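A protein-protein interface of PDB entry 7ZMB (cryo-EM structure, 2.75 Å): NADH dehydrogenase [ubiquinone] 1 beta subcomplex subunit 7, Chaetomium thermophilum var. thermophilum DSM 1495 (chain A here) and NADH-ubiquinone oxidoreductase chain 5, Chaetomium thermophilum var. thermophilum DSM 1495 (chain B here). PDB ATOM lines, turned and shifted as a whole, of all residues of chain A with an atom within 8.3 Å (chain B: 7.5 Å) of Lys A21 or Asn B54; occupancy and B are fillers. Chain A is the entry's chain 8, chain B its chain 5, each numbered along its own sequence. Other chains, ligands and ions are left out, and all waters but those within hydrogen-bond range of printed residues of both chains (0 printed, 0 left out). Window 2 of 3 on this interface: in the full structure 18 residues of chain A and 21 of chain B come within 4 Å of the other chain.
Hydrophobic or aromatic side chains of chain B within 4 Å of the printed part of chain A: Phe B52 and Val B501.
Along chain B the printed residues that touch a printed residue of chain A span positions 52 to 501.
Printed residues of chain A that touch a printed residue of chain B: Lys A21, Pro A23, Asn A38, Tyr A42 and Tyr A46.
Along chain A the printed residues that touch a printed residue of chain B span positions 21 to 46.
Among the printed residues, 9 pairs touch across the chains.
Among the printed residues, no Asp or Glu carboxylate lies within 4 Å of a Lys or Arg side-chain nitrogen of the other chain.
Among the printed residues, pairs that only touch across the chains: Tyr A46 with Phe B499, Tyr A42 with Asn B53, Lys A21 with Val B501, Lys A21 with Asn B54, Tyr A42 with Phe B52, Pro A23 with Ser B497 and Tyr A46 with Phe B52.
Met A17 touches none of the printed residues of chain B.
Ala A20 touches none of the printed residues of chain B.
Of the printed residues of chain B, Lys A21 touches Asn B54 (3.7 Å) and Val B501 (3.7 Å).
Of the printed residues of chain B, Asn A38 touches Asn B498.
Of the printed residues of chain A, Asn B53 touches Tyr A42 (3.6 Å).
Asn B54 touches just one residue of chain A: Lys A21 (3.7 Å).
Ser B80 touches none of the printed residues of chain A.
The nearest residue of chain B that does not touch Lys A21 is Asn B498 (4.4 Å).
The nearest printed residue of chain A that does not touch Phe B52 is Asn A38 (7.9 Å).
The side-chain amide nitrogen (ND2) of Asn A38 lies close to the side-chain amide nitrogen (ND2) of Asn B498 (3.3 Å).
O of Asn B498 sits close to OH of Tyr A46 (3.5 Å).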
ATOM      1  N   ARG A  14     -32.083  45.019 -17.081  1.00  0.00           N
ATOM      2  CA  ARG A  14     -31.640  43.913 -16.236  1.00  0.00           C
ATOM      3  C   ARG A  14     -32.711  42.841 -16.106  1.00  0.00           C
ATOM      4  O   ARG A  14     -32.418  41.647 -16.223  1.00  0.00           O
ATOM      5  CB  ARG A  14     -31.252  44.420 -14.847  1.00  0.00           C
ATOM      6  CG  ARG A  14     -29.878  45.049 -14.742  1.00  0.00           C
ATOM      7  CD  ARG A  14     -29.835  46.442 -15.329  1.00  0.00           C
ATOM      8  NE  ARG A  14     -28.515  47.035 -15.159  1.00  0.00           N
ATOM      9  CZ  ARG A  14     -28.139  47.712 -14.079  1.00  0.00           C
ATOM     10  NH1 ARG A  14     -26.917  48.216 -14.006  1.00  0.00           N
ATOM     11  NH2 ARG A  14     -28.984  47.879 -13.072  1.00  0.00           N
ATOM     12  N   GLU A  16     -34.992  41.732 -17.989  1.00  0.00           N
ATOM     13  CA  GLU A  16     -35.047  40.834 -19.135  1.00  0.00           C
ATOM     14  C   GLU A  16     -33.693  40.246 -19.500  1.00  0.00           C
ATOM     15  O   GLU A  16     -33.639  39.164 -20.093  1.00  0.00           O
ATOM     16  CB  GLU A  16     -35.622  41.562 -20.356  1.00  0.00           C
ATOM     17  CG  GLU A  16     -34.742  42.684 -20.882  1.00  0.00           C
ATOM     18  CD  GLU A  16     -35.315  43.346 -22.116  1.00  0.00           C
ATOM     19  OE1 GLU A  16     -36.376  42.895 -22.597  1.00  0.00           O
ATOM     20  OE2 GLU A  16     -34.704  44.318 -22.606  1.00  0.00           O
ATOM     21  N   MET A  17     -32.600  40.929 -19.159  1.00  0.00           N
ATOM     22  CA  MET A  17     -31.274  40.461 -19.547  1.00  0.00           C
ATOM     23  C   MET A  17     -30.682  39.512 -18.513  1.00  0.00           C
ATOM     24  O   MET A  17     -29.890  38.633 -18.869  1.00  0.00           O
ATOM     25  CB  MET A  17     -30.367  41.670 -19.800  1.00  0.00           C
ATOM     26  CG  MET A  17     -28.954  41.377 -20.277  1.00  0.00           C
ATOM     27  SD  MET A  17     -27.819  40.965 -18.946  1.00  0.00           S
ATOM     28  CE  MET A  17     -27.626  42.575 -18.186  1.00  0.00           C
ATOM     29  N   ARG A  18     -31.058  39.659 -17.240  1.00  0.00           N
ATOM     30  CA  ARG A  18     -30.610  38.706 -16.229  1.00  0.00           C
ATOM     31  C   ARG A  18     -31.173  37.316 -16.493  1.00  0.00           C
ATOM     32  O   ARG A  18     -30.473  36.312 -16.312  1.00  0.00           O
ATOM     33  CB  ARG A  18     -31.007  39.190 -14.834  1.00  0.00           C
ATOM     34  CG  ARG A  18     -30.558  38.277 -13.705  1.00  0.00           C
ATOM     35  CD  ARG A  18     -31.725  37.498 -13.116  1.00  0.00           C
ATOM     36  NE  ARG A  18     -32.876  38.351 -12.838  1.00  0.00           N
ATOM     37  CZ  ARG A  18     -32.966  39.171 -11.796  1.00  0.00           C
ATOM     38  NH1 ARG A  18     -34.055  39.909 -11.625  1.00  0.00           N
ATOM     39  NH2 ARG A  18     -31.971  39.258 -10.925  1.00  0.00           N
ATOM     40  N   ASP A  19     -32.435  37.237 -16.920  1.00  0.00           N
ATOM     41  CA  ASP A  19     -33.041  35.946 -17.220  1.00  0.00           C
ATOM     42  C   ASP A  19     -32.360  35.250 -18.390  1.00  0.00           C
ATOM     43  O   ASP A  19     -32.443  34.022 -18.500  1.00  0.00           O
ATOM     44  CB  ASP A  19     -34.532  36.122 -17.514  1.00  0.00           C
ATOM     45  CG  ASP A  19     -35.324  36.519 -16.283  1.00  0.00           C
ATOM     46  OD1 ASP A  19     -34.913  36.143 -15.166  1.00  0.00           O
ATOM     47  OD2 ASP A  19     -36.355  37.207 -16.435  1.00  0.00           O
ATOM     48  N   ALA A  20     -31.691  36.004 -19.264  1.00  0.00           N
ATOM     49  CA  ALA A  20     -30.943  35.393 -20.355  1.00  0.00           C
ATOM     50  C   ALA A  20     -29.719  34.636 -19.859  1.00  0.00           C
ATOM     51  O   ALA A  20     -29.193  33.791 -20.591  1.00  0.00           O
ATOM     52  CB  ALA A  20     -30.521  36.458 -21.366  1.00  0.00           C
ATOM     53  N   LYS A  21     -29.259  34.921 -18.638  1.00  0.00           N
ATOM     54  CA  LYS A  21     -28.138  34.222 -18.010  1.00  0.00           C
ATOM     55  C   LYS A  21     -26.876  34.341 -18.875  1.00  0.00           C
ATOM     56  O   LYS A  21     -26.364  33.374 -19.440  1.00  0.00           O
ATOM     57  CB  LYS A  21     -28.503  32.758 -17.729  1.00  0.00           C
ATOM     58  CG  LYS A  21     -27.455  31.975 -16.953  1.00  0.00           C
ATOM     59  CD  LYS A  21     -27.868  30.524 -16.779  1.00  0.00           C
ATOM     60  CE  LYS A  21     -28.981  30.383 -15.756  1.00  0.00           C
ATOM     61  NZ  LYS A  21     -29.308  28.955 -15.497  1.00  0.00           N
ATOM     62  N   VAL A  22     -26.409  35.581 -18.985  1.00  0.00           N
ATOM     63  CA  VAL A  22     -25.211  35.893 -19.758  1.00  0.00           C
ATOM     64  C   VAL A  22     -24.069  36.176 -18.787  1.00  0.00           C
ATOM     65  O   VAL A  22     -24.322  36.544 -17.631  1.00  0.00           O
ATOM     66  CB  VAL A  22     -25.460  37.075 -20.707  1.00  0.00           C
ATOM     67  CG1 VAL A  22     -26.658  36.786 -21.594  1.00  0.00           C
ATOM     68  CG2 VAL A  22     -25.668  38.349 -19.923  1.00  0.00           C
ATOM     69  N   PRO A  23     -22.811  36.012 -19.197  1.00  0.00           N
ATOM     70  CA  PRO A  23     -21.697  36.177 -18.256  1.00  0.00           C
ATOM     71  C   PRO A  23     -21.597  37.600 -17.722  1.00  0.00           C
ATOM     72  O   PRO A  23     -22.081  38.559 -18.326  1.00  0.00           O
ATOM     73  CB  PRO A  23     -20.465  35.814 -19.093  1.00  0.00           C
ATOM     74  CG  PRO A  23     -20.996  34.963 -20.193  1.00  0.00           C
ATOM     75  CD  PRO A  23     -22.354  35.505 -20.502  1.00  0.00           C
ATOM     76  N   LEU A  24     -20.953  37.718 -16.556  1.00  0.00           N
ATOM     77  CA  LEU A  24     -20.833  39.016 -15.899  1.00  0.00           C
ATOM     78  C   LEU A  24     -20.052  40.004 -16.755  1.00  0.00           C
ATOM     79  O   LEU A  24     -20.421  41.180 -16.853  1.00  0.00           O
ATOM     80  CB  LEU A  24     -20.158  38.870 -14.534  1.00  0.00           C
ATOM     81  CG  LEU A  24     -20.982  38.451 -13.315  1.00  0.00           C
ATOM     82  CD1 LEU A  24     -22.108  39.441 -13.049  1.00  0.00           C
ATOM     83  CD2 LEU A  24     -21.505  37.039 -13.441  1.00  0.00           C
ATOM     84  N   ARG A  27     -22.250  41.845 -19.410  1.00  0.00           N
ATOM     85  CA  ARG A  27     -23.489  42.499 -19.008  1.00  0.00           C
ATOM     86  C   ARG A  27     -23.614  43.917 -19.547  1.00  0.00           C
ATOM     87  O   ARG A  27     -24.524  44.640 -19.129  1.00  0.00           O
ATOM     88  CB  ARG A  27     -23.610  42.532 -17.482  1.00  0.00           C
ATOM     89  CG  ARG A  27     -23.642  41.178 -16.801  1.00  0.00           C
ATOM     90  CD  ARG A  27     -24.929  40.460 -17.135  1.00  0.00           C
ATOM     91  NE  ARG A  27     -25.027  39.144 -16.517  1.00  0.00           N
ATOM     92  CZ  ARG A  27     -25.561  38.930 -15.319  1.00  0.00           C
ATOM     93  NH1 ARG A  27     -26.042  39.947 -14.618  1.00  0.00           N
ATOM     94  NH2 ARG A  27     -25.619  37.705 -14.822  1.00  0.00           N
ATOM     95  N   LEU A  34     -26.315  39.876 -28.049  1.00  0.00           N
ATOM     96  CA  LEU A  34     -25.706  38.662 -27.522  1.00  0.00           C
ATOM     97  C   LEU A  34     -26.751  37.620 -27.145  1.00  0.00           C
ATOM     98  O   LEU A  34     -26.492  36.418 -27.274  1.00  0.00           O
ATOM     99  CB  LEU A  34     -24.821  39.004 -26.319  1.00  0.00           C
ATOM    100  CG  LEU A  34     -23.927  37.932 -25.689  1.00  0.00           C
ATOM    101  CD1 LEU A  34     -22.730  38.588 -25.024  1.00  0.00           C
ATOM    102  CD2 LEU A  34     -24.679  37.106 -24.665  1.00  0.00           C
ATOM    103  N   ILE A  35     -27.924  38.056 -26.680  1.00  0.00           N
ATOM    104  CA  ILE A  35     -28.972  37.105 -26.304  1.00  0.00           C
ATOM    105  C   ILE A  35     -29.388  36.220 -27.474  1.00  0.00           C
ATOM    106  O   ILE A  35     -29.457  34.993 -27.295  1.00  0.00           O
ATOM    107  CB  ILE A  35     -30.159  37.851 -25.670  1.00  0.00           C
ATOM    108  CG1 ILE A  35     -29.666  38.803 -24.580  1.00  0.00           C
ATOM    109  CG2 ILE A  35     -31.171  36.862 -25.115  1.00  0.00           C
ATOM    110  CD1 ILE A  35     -30.767  39.354 -23.704  1.00  0.00           C
ATOM    111  N   ASN A  38     -26.466  33.660 -28.175  1.00  0.00           N
ATOM    112  CA  ASN A  38     -26.380  32.520 -27.271  1.00  0.00           C
ATOM    113  C   ASN A  38     -27.396  31.447 -27.630  1.00  0.00           C
ATOM    114  O   ASN A  38     -27.163  30.261 -27.372  1.00  0.00           O
ATOM    115  CB  ASN A  38     -26.588  32.975 -25.828  1.00  0.00           C
ATOM    116  CG  ASN A  38     -25.341  33.580 -25.225  1.00  0.00           C
ATOM    117  OD1 ASN A  38     -24.298  33.666 -25.873  1.00  0.00           O
ATOM    118  ND2 ASN A  38     -25.440  34.004 -23.970  1.00  0.00           N
ATOM    119  N   TYR A  42     -26.853  27.321 -28.488  1.00  0.00           N
ATOM    120  CA  TYR A  42     -27.738  26.363 -27.837  1.00  0.00           C
ATOM    121  C   TYR A  42     -28.512  25.546 -28.861  1.00  0.00           C
ATOM    122  O   TYR A  42     -28.781  24.359 -28.644  1.00  0.00           O
ATOM    123  CB  TYR A  42     -28.687  27.102 -26.894  1.00  0.00           C
ATOM    124  CG  TYR A  42     -29.634  26.213 -26.127  1.00  0.00           C
ATOM    125  CD1 TYR A  42     -29.194  25.466 -25.045  1.00  0.00           C
ATOM    126  CD2 TYR A  42     -30.978  26.146 -26.467  1.00  0.00           C
ATOM    127  CE1 TYR A  42     -30.061  24.659 -24.336  1.00  0.00           C
ATOM    128  CE2 TYR A  42     -31.853  25.344 -25.763  1.00  0.00           C
ATOM    129  CZ  TYR A  42     -31.389  24.602 -24.699  1.00  0.00           C
ATOM    130  OH  TYR A  42     -32.257  23.801 -23.996  1.00  0.00           O
ATOM    131  N   TYR A  46     -23.137  24.607 -30.580  1.00  0.00           N
ATOM    132  CA  TYR A  46     -21.977  25.486 -30.691  1.00  0.00           C
ATOM    133  C   TYR A  46     -21.102  25.168 -31.902  1.00  0.00           C
ATOM    134  O   TYR A  46     -19.903  25.463 -31.894  1.00  0.00           O
ATOM    135  CB  TYR A  46     -21.122  25.442 -29.418  1.00  0.00           C
ATOM    136  CG  TYR A  46     -21.735  26.086 -28.194  1.00  0.00           C
ATOM    137  CD1 TYR A  46     -22.945  25.643 -27.678  1.00  0.00           C
ATOM    138  CD2 TYR A  46     -21.090  27.126 -27.544  1.00  0.00           C
ATOM    139  CE1 TYR A  46     -23.500  26.228 -26.558  1.00  0.00           C
ATOM    140  CE2 TYR A  46     -21.636  27.716 -26.423  1.00  0.00           C
ATOM    141  CZ  TYR A  46     -22.840  27.263 -25.934  1.00  0.00           C
ATOM    142  OH  TYR A  46     -23.386  27.851 -24.816  1.00  0.00           O
ATOM    143  N   PHE B  47     -20.947  15.155 -21.126  1.00  0.00           N
ATOM    144  CA  PHE B  47     -20.547  16.405 -21.755  1.00  0.00           C
ATOM    145  C   PHE B  47     -21.664  16.959 -22.628  1.00  0.00           C
ATOM    146  O   PHE B  47     -21.902  18.172 -22.651  1.00  0.00           O
ATOM    147  CB  PHE B  47     -19.275  16.195 -22.572  1.00  0.00           C
ATOM    148  CG  PHE B  47     -18.631  17.468 -23.023  1.00  0.00           C
ATOM    149  CD1 PHE B  47     -17.792  18.171 -22.178  1.00  0.00           C
ATOM    150  CD2 PHE B  47     -18.859  17.959 -24.296  1.00  0.00           C
ATOM    151  CE1 PHE B  47     -17.196  19.340 -22.593  1.00  0.00           C
ATOM    152  CE2 PHE B  47     -18.266  19.130 -24.717  1.00  0.00           C
ATOM    153  CZ  PHE B  47     -17.433  19.821 -23.866  1.00  0.00           C
ATOM    154  N   PHE B  48     -22.357  16.087 -23.363  1.00  0.00           N
ATOM    155  CA  PHE B  48     -23.513  16.531 -24.133  1.00  0.00           C
ATOM    156  C   PHE B  48     -24.684  16.926 -23.249  1.00  0.00           C
ATOM    157  O   PHE B  48     -25.544  17.694 -23.693  1.00  0.00           O
ATOM    158  CB  PHE B  48     -23.956  15.448 -25.117  1.00  0.00           C
ATOM    159  CG  PHE B  48     -23.025  15.266 -26.284  1.00  0.00           C
ATOM    160  CD1 PHE B  48     -22.077  16.227 -26.590  1.00  0.00           C
ATOM    161  CD2 PHE B  48     -23.117  14.144 -27.089  1.00  0.00           C
ATOM    162  CE1 PHE B  48     -21.227  16.064 -27.669  1.00  0.00           C
ATOM    163  CE2 PHE B  48     -22.270  13.977 -28.169  1.00  0.00           C
ATOM    164  CZ  PHE B  48     -21.324  14.939 -28.459  1.00  0.00           C
ATOM    165  N   GLU B  49     -24.748  16.425 -22.015  1.00  0.00           N
ATOM    166  CA  GLU B  49     -25.863  16.747 -21.131  1.00  0.00           C
ATOM    167  C   GLU B  49     -25.543  17.831 -20.107  1.00  0.00           C
ATOM    168  O   GLU B  49     -26.346  18.745 -19.904  1.00  0.00           O
ATOM    169  CB  GLU B  49     -26.390  15.498 -20.421  1.00  0.00           C
ATOM    170  CG  GLU B  49     -27.545  15.900 -19.553  1.00  0.00           C
ATOM    171  CD  GLU B  49     -28.713  16.421 -20.365  1.00  0.00           C
ATOM    172  OE1 GLU B  49     -28.863  16.038 -21.544  1.00  0.00           O
ATOM    173  OE2 GLU B  49     -29.407  17.321 -19.859  1.00  0.00           O
ATOM    174  N   VAL B  50     -24.397  17.744 -19.439  1.00  0.00           N
ATOM    175  CA  VAL B  50     -24.083  18.739 -18.420  1.00  0.00           C
ATOM    176  C   VAL B  50     -23.819  20.096 -19.060  1.00  0.00           C
ATOM    177  O   VAL B  50     -24.352  21.123 -18.624  1.00  0.00           O
ATOM    178  CB  VAL B  50     -22.891  18.283 -17.568  1.00  0.00           C
ATOM    179  CG1 VAL B  50     -22.532  19.368 -16.607  1.00  0.00           C
ATOM    180  CG2 VAL B  50     -23.223  17.002 -16.825  1.00  0.00           C
ATOM    181  N   GLY B  51     -23.000  20.120 -20.106  1.00  0.00           N
ATOM    182  CA  GLY B  51     -22.570  21.374 -20.690  1.00  0.00           C
ATOM    183  C   GLY B  51     -23.509  21.955 -21.724  1.00  0.00           C
ATOM    184  O   GLY B  51     -23.959  23.097 -21.587  1.00  0.00           O
ATOM    185  N   PHE B  52     -23.815  21.180 -22.766  1.00  0.00           N
ATOM    186  CA  PHE B  52     -24.585  21.714 -23.885  1.00  0.00           C
ATOM    187  C   PHE B  52     -25.982  22.135 -23.452  1.00  0.00           C
ATOM    188  O   PHE B  52     -26.479  23.186 -23.871  1.00  0.00           O
ATOM    189  CB  PHE B  52     -24.653  20.686 -25.009  1.00  0.00           C
ATOM    190  CG  PHE B  52     -23.476  20.734 -25.935  1.00  0.00           C
ATOM    191  CD1 PHE B  52     -23.024  21.942 -26.436  1.00  0.00           C
ATOM    192  CD2 PHE B  52     -22.807  19.578 -26.284  1.00  0.00           C
ATOM    193  CE1 PHE B  52     -21.937  21.993 -27.281  1.00  0.00           C
ATOM    194  CE2 PHE B  52     -21.718  19.622 -27.127  1.00  0.00           C
ATOM    195  CZ  PHE B  52     -21.281  20.830 -27.626  1.00  0.00           C
ATOM    196  N   ASN B  53     -26.629  21.333 -22.617  1.00  0.00           N
ATOM    197  CA  ASN B  53     -27.957  21.661 -22.128  1.00  0.00           C
ATOM    198  C   ASN B  53     -27.941  22.480 -20.844  1.00  0.00           C
ATOM    199  O   ASN B  53     -28.995  22.980 -20.438  1.00  0.00           O
ATOM    200  CB  ASN B  53     -28.758  20.379 -21.913  1.00  0.00           C
ATOM    201  CG  ASN B  53     -29.534  19.969 -23.138  1.00  0.00           C
ATOM    202  OD1 ASN B  53     -30.433  20.683 -23.579  1.00  0.00           O
ATOM    203  ND2 ASN B  53     -29.193  18.816 -23.698  1.00  0.00           N
ATOM    204  N   ASN B  54     -26.777  22.640 -20.216  1.00  0.00           N
ATOM    205  CA  ASN B  54     -26.622  23.405 -18.977  1.00  0.00           C
ATOM    206  C   ASN B  54     -27.503  22.803 -17.876  1.00  0.00           C
ATOM    207  O   ASN B  54     -28.483  23.392 -17.418  1.00  0.00           O
ATOM    208  CB  ASN B  54     -26.922  24.894 -19.227  1.00  0.00           C
ATOM    209  CG  ASN B  54     -27.030  25.723 -17.947  1.00  0.00           C
ATOM    210  OD1 ASN B  54     -26.657  25.284 -16.859  1.00  0.00           O
ATOM    211  ND2 ASN B  54     -27.558  26.933 -18.082  1.00  0.00           N
ATOM    212  N   ILE B  55     -27.167  21.574 -17.498  1.00  0.00           N
ATOM    213  CA  ILE B  55     -27.713  20.950 -16.294  1.00  0.00           C
ATOM    214  C   ILE B  55     -26.585  20.337 -15.481  1.00  0.00           C
ATOM    215  O   ILE B  55     -26.107  19.241 -15.809  1.00  0.00           O
ATOM    216  CB  ILE B  55     -28.778  19.882 -16.595  1.00  0.00           C
ATOM    217  CG1 ILE B  55     -30.002  20.473 -17.279  1.00  0.00           C
ATOM    218  CG2 ILE B  55     -29.198  19.194 -15.323  1.00  0.00           C
ATOM    219  CD1 ILE B  55     -29.927  20.510 -18.742  1.00  0.00           C
ATOM    220  N   PRO B  56     -26.126  21.001 -14.429  1.00  0.00           N
ATOM    221  CA  PRO B  56     -25.241  20.342 -13.474  1.00  0.00           C
ATOM    222  C   PRO B  56     -26.024  19.413 -12.559  1.00  0.00           C
ATOM    223  O   PRO B  56     -27.159  19.694 -12.171  1.00  0.00           O
ATOM    224  CB  PRO B  56     -24.626  21.515 -12.703  1.00  0.00           C
ATOM    225  CG  PRO B  56     -25.630  22.573 -12.781  1.00  0.00           C
ATOM    226  CD  PRO B  56     -26.384  22.401 -14.070  1.00  0.00           C
ATOM    227  N   SER B  80     -20.006  22.214 -15.866  1.00  0.00           N
ATOM    228  CA  SER B  80     -19.365  22.391 -17.162  1.00  0.00           C
ATOM    229  C   SER B  80     -17.880  22.077 -17.109  1.00  0.00           C
ATOM    230  O   SER B  80     -17.317  21.583 -18.089  1.00  0.00           O
ATOM    231  CB  SER B  80     -19.592  23.816 -17.667  1.00  0.00           C
ATOM    232  OG  SER B  80     -18.741  24.725 -16.999  1.00  0.00           O
ATOM    233  N   SER B 497     -19.378  33.323 -25.359  1.00  0.00           N
ATOM    234  CA  SER B 497     -19.919  31.994 -25.118  1.00  0.00           C
ATOM    235  C   SER B 497     -20.558  31.907 -23.740  1.00  0.00           C
ATOM    236  O   SER B 497     -20.014  32.405 -22.749  1.00  0.00           O
ATOM    237  CB  SER B 497     -18.818  30.944 -25.248  1.00  0.00           C
ATOM    238  OG  SER B 497     -17.983  30.948 -24.105  1.00  0.00           O
ATOM    239  N   ASN B 498     -21.723  31.270 -23.686  1.00  0.00           N
ATOM    240  CA  ASN B 498     -22.458  31.053 -22.448  1.00  0.00           C
ATOM    241  C   ASN B 498     -22.400  29.589 -22.033  1.00  0.00           C
ATOM    242  O   ASN B 498     -23.374  29.023 -21.535  1.00  0.00           O
ATOM    243  CB  ASN B 498     -23.905  31.517 -22.583  1.00  0.00           C
ATOM    244  CG  ASN B 498     -24.700  30.683 -23.570  1.00  0.00           C
ATOM    245  OD1 ASN B 498     -24.135  29.966 -24.396  1.00  0.00           O
ATOM    246  ND2 ASN B 498     -26.022  30.760 -23.473  1.00  0.00           N
ATOM    247  N   PHE B 499     -21.253  28.951 -22.258  1.00  0.00           N
ATOM    248  CA  PHE B 499     -21.104  27.559 -21.860  1.00  0.00           C
ATOM    249  C   PHE B 499     -20.906  27.442 -20.354  1.00  0.00           C
ATOM    250  O   PHE B 499     -21.356  26.471 -19.735  1.00  0.00           O
ATOM    251  CB  PHE B 499     -19.930  26.936 -22.617  1.00  0.00           C
ATOM    252  CG  PHE B 499     -19.818  25.449 -22.459  1.00  0.00           C
ATOM    253  CD1 PHE B 499     -20.691  24.604 -23.119  1.00  0.00           C
ATOM    254  CD2 PHE B 499     -18.826  24.896 -21.671  1.00  0.00           C
ATOM    255  CE1 PHE B 499     -20.587  23.237 -22.985  1.00  0.00           C
ATOM    256  CE2 PHE B 499     -18.718  23.527 -21.533  1.00  0.00           C
ATOM    257  CZ  PHE B 499     -19.600  22.697 -22.192  1.00  0.00           C
ATOM    258  N   PHE B 500     -20.237  28.420 -19.752  1.00  0.00           N
ATOM    259  CA  PHE B 500     -19.856  28.365 -18.342  1.00  0.00           C
ATOM    260  C   PHE B 500     -20.794  29.221 -17.489  1.00  0.00           C
ATOM    261  O   PHE B 500     -20.361  30.109 -16.759  1.00  0.00           O
ATOM    262  CB  PHE B 500     -18.412  28.829 -18.190  1.00  0.00           C
ATOM    263  CG  PHE B 500     -17.420  27.912 -18.831  1.00  0.00           C
ATOM    264  CD1 PHE B 500     -17.002  26.765 -18.198  1.00  0.00           C
ATOM    265  CD2 PHE B 500     -16.919  28.198 -20.088  1.00  0.00           C
ATOM    266  CE1 PHE B 500     -16.097  25.917 -18.801  1.00  0.00           C
ATOM    267  CE2 PHE B 500     -16.010  27.358 -20.693  1.00  0.00           C
ATOM    268  CZ  PHE B 500     -15.600  26.217 -20.048  1.00  0.00           C
ATOM    269  N   VAL B 501     -22.096  28.949 -17.568  1.00  0.00           N
ATOM    270  CA  VAL B 501     -23.091  29.830 -16.965  1.00  0.00           C
ATOM    271  C   VAL B 501     -23.659  29.276 -15.667  1.00  0.00           C
ATOM    272  O   VAL B 501     -24.640  29.817 -15.149  1.00  0.00           O
ATOM    273  CB  VAL B 501     -24.221  30.173 -17.944  1.00  0.00           C
ATOM    274  CG1 VAL B 501     -23.666  30.917 -19.122  1.00  0.00           C
ATOM    275  CG2 VAL B 501     -24.927  28.905 -18.394  1.00  0.00           C
ATOM    276  N   ASP B 502     -23.075  28.216 -15.118  1.00  0.00           N
ATOM    277  CA  ASP B 502     -23.468  27.738 -13.800  1.00  0.00           C
ATOM    278  C   ASP B 502     -22.437  28.112 -12.742  1.00  0.00           C
ATOM    279  O   ASP B 502     -22.328  27.451 -11.706  1.00  0.00           O
ATOM    280  CB  ASP B 502     -23.729  26.232 -13.827  1.00  0.00           C
ATOM    281  CG  ASP B 502     -22.502  25.425 -14.189  1.00  0.00           C
ATOM    282  OD1 ASP B 502     -21.446  26.023 -14.465  1.00  0.00           O
ATOM    283  OD2 ASP B 502     -22.597  24.182 -14.197  1.00  0.00           O
ATOM    284  N   ASN B 503     -21.700  29.194 -12.988  1.00  0.00           N
ATOM    285  CA  ASN B 503     -20.590  29.629 -12.140  1.00  0.00           C
ATOM    286  C   ASN B 503     -19.597  28.494 -11.932  1.00  0.00           C
ATOM    287  O   ASN B 503     -19.214  28.158 -10.812  1.00  0.00           O
ATOM    288  CB  ASN B 503     -21.081  30.182 -10.804  1.00  0.00           C
ATOM    289  CG  ASN B 503     -20.063  31.095 -10.144  1.00  0.00           C
ATOM    290  OD1 ASN B 503     -18.988  30.657  -9.750  1.00  0.00           O
ATOM    291  ND2 ASN B 503     -20.401  32.370 -10.022  1.00  0.00           N
